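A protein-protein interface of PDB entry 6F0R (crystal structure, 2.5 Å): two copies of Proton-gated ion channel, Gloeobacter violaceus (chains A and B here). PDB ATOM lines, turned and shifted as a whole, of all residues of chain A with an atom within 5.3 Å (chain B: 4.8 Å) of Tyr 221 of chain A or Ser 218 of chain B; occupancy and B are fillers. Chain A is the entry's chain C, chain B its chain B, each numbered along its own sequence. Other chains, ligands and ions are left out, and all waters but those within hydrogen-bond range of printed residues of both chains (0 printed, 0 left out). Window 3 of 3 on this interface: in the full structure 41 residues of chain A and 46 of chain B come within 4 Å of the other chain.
The backbone NH of Ser 220 of chain B sits at hydrogen-bond distance from the side-chain hydroxyl of Ser 218 of chain B (3.2 Å). The backbone carbonyl oxygen of Ser 220 of chain B sits close to the side-chain amide oxygen of Asn 224 of chain B (3.2 Å). O of Glu 222 of chain A sits at hydrogen-bond distance from OG1 of Thr 226 of chain A, at 3.2 Å. The backbone carbonyl oxygen of Ser 218 of chain B sits at hydrogen-bond distance from the side-chain amide nitrogen of Gln 276 of chain B, 2.8 Å away. The side-chain amide oxygen of Asn 224 of chain B lies within hydrogen-bond range of the side-chain hydroxyl of Ser 218 of chain B, at 2.7 Å.
Tyr 221 of chain A touches four residues of chain B. Printed residues of chain B within 4 Å of Thr 274 of chain A: Thr 214 (3.5 Å) and Trp 217 (3.8 Å). Ser 218 of chain B touches one residue of chain A. Printed residues of chain A within 4 Å of Ser 220 of chain B: Tyr 221 (3.9 Å) and Glu 222 (3.0 Å). Of the printed residues of chain A, Ala 223 of chain B touches Tyr 221 and Val 225.
Hydrophobic or aromatic side chains of chain B that line the printed part of chain A: Trp 217, Ala 223 and Leu 227. Among the printed residues, no Asp or Glu carboxylate lies within 4 Å of a Lys or Arg side-chain nitrogen of the other chain.
The side-chain hydroxyl (OG) of Ser 220 of chain B lies within hydrogen-bond range of the side-chain carboxylate (OE2) of Glu 222 of chain A (3.0 Å).
Ser 218 of chain B touches Tyr 221 of chain A. Tyr 221 of chain A touches Ser 220 of chain B (CD2 to CB, 3.9 Å). Tyr 221 of chain A touches Ala 223 of chain B (CE2 to CB, 3.4 Å). Tyr 221 of chain A touches Leu 227 of chain B. Val 225 of chain A touches Ala 223 of chain B. OG1 of Thr 274 of chain A touches CB of Thr 214 of chain B, 3.5 Å away. CG2 of Thr 274 of chain A touches CB of Trp 217 of chain B, 3.8 Å away.
Positions printed for both chains: 218, 219, 220, 223 and 224. Of the 8 pairs that touch across the chains among the printed residues, none has its exchanged pair printed and touching as well.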
ATOM      1  N   SER A 218     -31.638  33.099  20.213  1.00  0.00           N
ATOM      2  CA  SER A 218     -30.641  33.950  19.615  1.00  0.00           C
ATOM      3  C   SER A 218     -30.503  33.610  18.154  1.00  0.00           C
ATOM      4  O   SER A 218     -30.475  32.427  17.785  1.00  0.00           O
ATOM      5  CB  SER A 218     -29.301  33.784  20.317  1.00  0.00           C
ATOM      6  OG  SER A 218     -28.244  34.266  19.506  1.00  0.00           O
ATOM      7  N   THR A 219     -30.414  34.679  17.330  1.00  0.00           N
ATOM      8  CA  THR A 219     -30.242  34.681  15.875  1.00  0.00           C
ATOM      9  C   THR A 219     -28.772  34.941  15.505  1.00  0.00           C
ATOM     10  O   THR A 219     -28.377  34.743  14.337  1.00  0.00           O
ATOM     11  CB  THR A 219     -31.188  35.688  15.221  1.00  0.00           C
ATOM     12  OG1 THR A 219     -31.483  36.736  16.154  1.00  0.00           O
ATOM     13  CG2 THR A 219     -32.477  35.052  14.793  1.00  0.00           C
ATOM     14  N   SER A 220     -27.961  35.315  16.529  1.00  0.00           N
ATOM     15  CA  SER A 220     -26.558  35.677  16.430  1.00  0.00           C
ATOM     16  C   SER A 220     -25.659  34.451  16.427  1.00  0.00           C
ATOM     17  O   SER A 220     -25.351  33.911  17.498  1.00  0.00           O
ATOM     18  CB  SER A 220     -26.200  36.612  17.575  1.00  0.00           C
ATOM     19  OG  SER A 220     -24.831  36.965  17.506  1.00  0.00           O
ATOM     20  N   TYR A 221     -25.209  34.015  15.229  1.00  0.00           N
ATOM     21  CA  TYR A 221     -24.333  32.851  15.040  1.00  0.00           C
ATOM     22  C   TYR A 221     -23.069  32.935  15.847  1.00  0.00           C
ATOM     23  O   TYR A 221     -22.703  31.958  16.503  1.00  0.00           O
ATOM     24  CB  TYR A 221     -24.003  32.652  13.564  1.00  0.00           C
ATOM     25  CG  TYR A 221     -23.196  31.408  13.237  1.00  0.00           C
ATOM     26  CD1 TYR A 221     -23.605  30.148  13.670  1.00  0.00           C
ATOM     27  CD2 TYR A 221     -22.083  31.476  12.406  1.00  0.00           C
ATOM     28  CE1 TYR A 221     -22.928  28.996  13.282  1.00  0.00           C
ATOM     29  CE2 TYR A 221     -21.360  30.336  12.069  1.00  0.00           C
ATOM     30  CZ  TYR A 221     -21.797  29.097  12.494  1.00  0.00           C
ATOM     31  OH  TYR A 221     -21.081  27.977  12.137  1.00  0.00           O
ATOM     32  N   GLU A 222     -22.408  34.096  15.818  1.00  0.00           N
ATOM     33  CA  GLU A 222     -21.146  34.361  16.513  1.00  0.00           C
ATOM     34  C   GLU A 222     -21.328  34.124  18.029  1.00  0.00           C
ATOM     35  O   GLU A 222     -20.539  33.389  18.631  1.00  0.00           O
ATOM     36  CB  GLU A 222     -20.626  35.788  16.193  1.00  0.00           C
ATOM     37  CG  GLU A 222     -20.486  36.156  14.707  1.00  0.00           C
ATOM     38  CD  GLU A 222     -21.725  36.313  13.817  1.00  0.00           C
ATOM     39  OE1 GLU A 222     -22.776  36.816  14.286  1.00  0.00           O
ATOM     40  OE2 GLU A 222     -21.622  35.952  12.622  1.00  0.00           O
ATOM     41  N   ALA A 223     -22.413  34.679  18.617  1.00  0.00           N
ATOM     42  CA  ALA A 223     -22.776  34.532  20.027  1.00  0.00           C
ATOM     43  C   ALA A 223     -23.137  33.080  20.365  1.00  0.00           C
ATOM     44  O   ALA A 223     -22.662  32.552  21.378  1.00  0.00           O
ATOM     45  CB  ALA A 223     -23.922  35.473  20.364  1.00  0.00           C
ATOM     46  N   ASN A 224     -23.943  32.424  19.495  1.00  0.00           N
ATOM     47  CA  ASN A 224     -24.358  31.016  19.605  1.00  0.00           C
ATOM     48  C   ASN A 224     -23.185  30.054  19.641  1.00  0.00           C
ATOM     49  O   ASN A 224     -23.207  29.125  20.417  1.00  0.00           O
ATOM     50  CB  ASN A 224     -25.279  30.645  18.441  1.00  0.00           C
ATOM     51  CG  ASN A 224     -26.582  31.319  18.543  1.00  0.00           C
ATOM     52  OD1 ASN A 224     -26.882  31.925  19.565  1.00  0.00           O
ATOM     53  ND2 ASN A 224     -27.338  31.325  17.458  1.00  0.00           N
ATOM     54  N   VAL A 225     -22.206  30.253  18.754  1.00  0.00           N
ATOM     55  CA  VAL A 225     -20.993  29.467  18.622  1.00  0.00           C
ATOM     56  C   VAL A 225     -20.193  29.590  19.934  1.00  0.00           C
ATOM     57  O   VAL A 225     -19.764  28.571  20.455  1.00  0.00           O
ATOM     58  CB  VAL A 225     -20.236  29.916  17.338  1.00  0.00           C
ATOM     59  CG1 VAL A 225     -18.729  29.740  17.458  1.00  0.00           C
ATOM     60  CG2 VAL A 225     -20.750  29.161  16.135  1.00  0.00           C
ATOM     61  N   THR A 226     -20.087  30.815  20.510  1.00  0.00           N
ATOM     62  CA  THR A 226     -19.415  31.097  21.781  1.00  0.00           C
ATOM     63  C   THR A 226     -20.158  30.384  22.918  1.00  0.00           C
ATOM     64  O   THR A 226     -19.514  29.683  23.696  1.00  0.00           O
ATOM     65  CB  THR A 226     -19.255  32.621  21.986  1.00  0.00           C
ATOM     66  OG1 THR A 226     -18.419  33.163  20.960  1.00  0.00           O
ATOM     67  CG2 THR A 226     -18.632  32.977  23.327  1.00  0.00           C
ATOM     68  N   VAL A 273     -27.482  25.284  15.572  1.00  0.00           N
ATOM     69  CA  VAL A 273     -26.894  26.618  15.411  1.00  0.00           C
ATOM     70  C   VAL A 273     -26.337  26.846  13.964  1.00  0.00           C
ATOM     71  O   VAL A 273     -26.559  27.926  13.386  1.00  0.00           O
ATOM     72  CB  VAL A 273     -25.853  26.822  16.536  1.00  0.00           C
ATOM     73  CG1 VAL A 273     -24.832  27.893  16.201  1.00  0.00           C
ATOM     74  CG2 VAL A 273     -26.546  27.109  17.865  1.00  0.00           C
ATOM     75  N   THR A 274     -25.679  25.808  13.380  1.00  0.00           N
ATOM     76  CA  THR A 274     -25.114  25.767  12.021  1.00  0.00           C
ATOM     77  C   THR A 274     -26.244  25.862  10.979  1.00  0.00           C
ATOM     78  O   THR A 274     -26.182  26.726  10.091  1.00  0.00           O
ATOM     79  CB  THR A 274     -24.224  24.503  11.849  1.00  0.00           C
ATOM     80  OG1 THR A 274     -23.236  24.449  12.896  1.00  0.00           O
ATOM     81  CG2 THR A 274     -23.525  24.447  10.490  1.00  0.00           C
ATOM     82  N   HIS A 277     -28.111  29.246  10.988  1.00  0.00           N
ATOM     83  CA  HIS A 277     -27.283  30.262  10.335  1.00  0.00           C
ATOM     84  C   HIS A 277     -27.293  30.110   8.826  1.00  0.00           C
ATOM     85  O   HIS A 277     -27.526  31.094   8.128  1.00  0.00           O
ATOM     86  CB  HIS A 277     -25.850  30.225  10.875  1.00  0.00           C
ATOM     87  CG  HIS A 277     -24.892  31.119  10.150  1.00  0.00           C
ATOM     88  ND1 HIS A 277     -25.008  32.501  10.197  1.00  0.00           N
ATOM     89  CD2 HIS A 277     -23.819  30.797   9.396  1.00  0.00           C
ATOM     90  CE1 HIS A 277     -24.024  32.976   9.451  1.00  0.00           C
ATOM     91  NE2 HIS A 277     -23.293  31.990   8.926  1.00  0.00           N
ATOM     92  N   THR B 214     -17.982  22.095  11.232  1.00  0.00           N
ATOM     93  CA  THR B 214     -19.214  22.829  10.950  1.00  0.00           C
ATOM     94  C   THR B 214     -18.836  24.158  10.295  1.00  0.00           C
ATOM     95  O   THR B 214     -19.693  24.785   9.679  1.00  0.00           O
ATOM     96  CB  THR B 214     -20.128  22.985  12.197  1.00  0.00           C
ATOM     97  OG1 THR B 214     -19.414  23.612  13.247  1.00  0.00           O
ATOM     98  CG2 THR B 214     -20.714  21.674  12.704  1.00  0.00           C
ATOM     99  N   ALA B 215     -17.528  24.549  10.360  1.00  0.00           N
ATOM    100  CA  ALA B 215     -16.945  25.762   9.759  1.00  0.00           C
ATOM    101  C   ALA B 215     -17.014  25.727   8.220  1.00  0.00           C
ATOM    102  O   ALA B 215     -16.867  26.774   7.549  1.00  0.00           O
ATOM    103  CB  ALA B 215     -15.508  25.931  10.220  1.00  0.00           C
ATOM    104  N   PHE B 216     -17.260  24.514   7.658  1.00  0.00           N
ATOM    105  CA  PHE B 216     -17.408  24.288   6.212  1.00  0.00           C
ATOM    106  C   PHE B 216     -18.838  24.601   5.734  1.00  0.00           C
ATOM    107  O   PHE B 216     -19.103  24.508   4.552  1.00  0.00           O
ATOM    108  CB  PHE B 216     -16.916  22.871   5.798  1.00  0.00           C
ATOM    109  CG  PHE B 216     -15.532  22.536   6.326  1.00  0.00           C
ATOM    110  CD1 PHE B 216     -14.508  23.484   6.309  1.00  0.00           C
ATOM    111  CD2 PHE B 216     -15.251  21.276   6.841  1.00  0.00           C
ATOM    112  CE1 PHE B 216     -13.247  23.189   6.836  1.00  0.00           C
ATOM    113  CE2 PHE B 216     -13.982  20.972   7.323  1.00  0.00           C
ATOM    114  CZ  PHE B 216     -12.985  21.930   7.315  1.00  0.00           C
ATOM    115  N   TRP B 217     -19.743  24.987   6.656  1.00  0.00           N
ATOM    116  CA  TRP B 217     -21.126  25.392   6.396  1.00  0.00           C
ATOM    117  C   TRP B 217     -21.371  26.801   7.010  1.00  0.00           C
ATOM    118  O   TRP B 217     -22.469  27.140   7.466  1.00  0.00           O
ATOM    119  CB  TRP B 217     -22.073  24.355   6.989  1.00  0.00           C
ATOM    120  CG  TRP B 217     -22.171  23.106   6.174  1.00  0.00           C
ATOM    121  CD1 TRP B 217     -23.034  22.858   5.142  1.00  0.00           C
ATOM    122  CD2 TRP B 217     -21.395  21.916   6.349  1.00  0.00           C
ATOM    123  NE1 TRP B 217     -22.831  21.585   4.656  1.00  0.00           N
ATOM    124  CE2 TRP B 217     -21.826  20.987   5.381  1.00  0.00           C
ATOM    125  CE3 TRP B 217     -20.359  21.549   7.223  1.00  0.00           C
ATOM    126  CZ2 TRP B 217     -21.260  19.708   5.271  1.00  0.00           C
ATOM    127  CZ3 TRP B 217     -19.811  20.274   7.123  1.00  0.00           C
ATOM    128  CH2 TRP B 217     -20.253  19.376   6.149  1.00  0.00           C
ATOM    129  N   SER B 218     -20.306  27.590   7.075  1.00  0.00           N
ATOM    130  CA  SER B 218     -20.305  28.920   7.639  1.00  0.00           C
ATOM    131  C   SER B 218     -19.388  29.810   6.832  1.00  0.00           C
ATOM    132  O   SER B 218     -18.275  29.395   6.455  1.00  0.00           O
ATOM    133  CB  SER B 218     -19.835  28.888   9.085  1.00  0.00           C
ATOM    134  OG  SER B 218     -19.456  30.183   9.526  1.00  0.00           O
ATOM    135  N   THR B 219     -19.882  31.038   6.569  1.00  0.00           N
ATOM    136  CA  THR B 219     -19.214  32.123   5.842  1.00  0.00           C
ATOM    137  C   THR B 219     -18.621  33.151   6.823  1.00  0.00           C
ATOM    138  O   THR B 219     -17.823  34.016   6.419  1.00  0.00           O
ATOM    139  CB  THR B 219     -20.182  32.770   4.845  1.00  0.00           C
ATOM    140  OG1 THR B 219     -21.526  32.655   5.332  1.00  0.00           O
ATOM    141  CG2 THR B 219     -20.087  32.133   3.484  1.00  0.00           C
ATOM    142  N   SER B 220     -18.984  32.998   8.127  1.00  0.00           N
ATOM    143  CA  SER B 220     -18.604  33.837   9.250  1.00  0.00           C
ATOM    144  C   SER B 220     -17.210  33.485   9.774  1.00  0.00           C
ATOM    145  O   SER B 220     -17.064  32.539  10.560  1.00  0.00           O
ATOM    146  CB  SER B 220     -19.661  33.728  10.343  1.00  0.00           C
ATOM    147  OG  SER B 220     -19.301  34.501  11.471  1.00  0.00           O
ATOM    148  N   ALA B 223     -16.798  33.420  13.686  1.00  0.00           N
ATOM    149  CA  ALA B 223     -17.395  32.193  14.205  1.00  0.00           C
ATOM    150  C   ALA B 223     -16.521  30.978  13.903  1.00  0.00           C
ATOM    151  O   ALA B 223     -16.264  30.168  14.803  1.00  0.00           O
ATOM    152  CB  ALA B 223     -18.789  32.011  13.629  1.00  0.00           C
ATOM    153  N   ASN B 224     -16.019  30.874  12.658  1.00  0.00           N
ATOM    154  CA  ASN B 224     -15.105  29.807  12.182  1.00  0.00           C
ATOM    155  C   ASN B 224     -13.830  29.726  12.983  1.00  0.00           C
ATOM    156  O   ASN B 224     -13.383  28.635  13.316  1.00  0.00           O
ATOM    157  CB  ASN B 224     -14.753  30.028  10.704  1.00  0.00           C
ATOM    158  CG  ASN B 224     -15.937  29.832   9.826  1.00  0.00           C
ATOM    159  OD1 ASN B 224     -16.965  29.339  10.268  1.00  0.00           O
ATOM    160  ND2 ASN B 224     -15.854  30.292   8.596  1.00  0.00           N
ATOM    161  N   LEU B 227     -14.741  28.338  16.363  1.00  0.00           N
ATOM    162  CA  LEU B 227     -14.996  26.891  16.246  1.00  0.00           C
ATOM    163  C   LEU B 227     -13.733  26.081  16.196  1.00  0.00           C
ATOM    164  O   LEU B 227     -13.630  25.113  16.941  1.00  0.00           O
ATOM    165  CB  LEU B 227     -15.838  26.538  14.990  1.00  0.00           C
ATOM    166  CG  LEU B 227     -17.350  26.653  15.066  1.00  0.00           C
ATOM    167  CD1 LEU B 227     -17.955  26.778  13.655  1.00  0.00           C
ATOM    168  CD2 LEU B 227     -17.955  25.489  15.785  1.00  0.00           C
ATOM    169  N   GLN B 276     -10.772  30.913   2.625  1.00  0.00           N
ATOM    170  CA  GLN B 276     -12.171  31.260   2.393  1.00  0.00           C
ATOM    171  C   GLN B 276     -12.442  32.744   2.680  1.00  0.00           C
ATOM    172  O   GLN B 276     -13.072  33.421   1.846  1.00  0.00           O
ATOM    173  CB  GLN B 276     -13.080  30.357   3.235  1.00  0.00           C
ATOM    174  CG  GLN B 276     -14.554  30.779   3.275  1.00  0.00           C
ATOM    175  CD  GLN B 276     -15.268  30.328   4.527  1.00  0.00           C
ATOM    176  OE1 GLN B 276     -14.721  30.378   5.681  1.00  0.00           O
ATOM    177  NE2 GLN B 276     -16.531  29.925   4.315  1.00  0.00           N
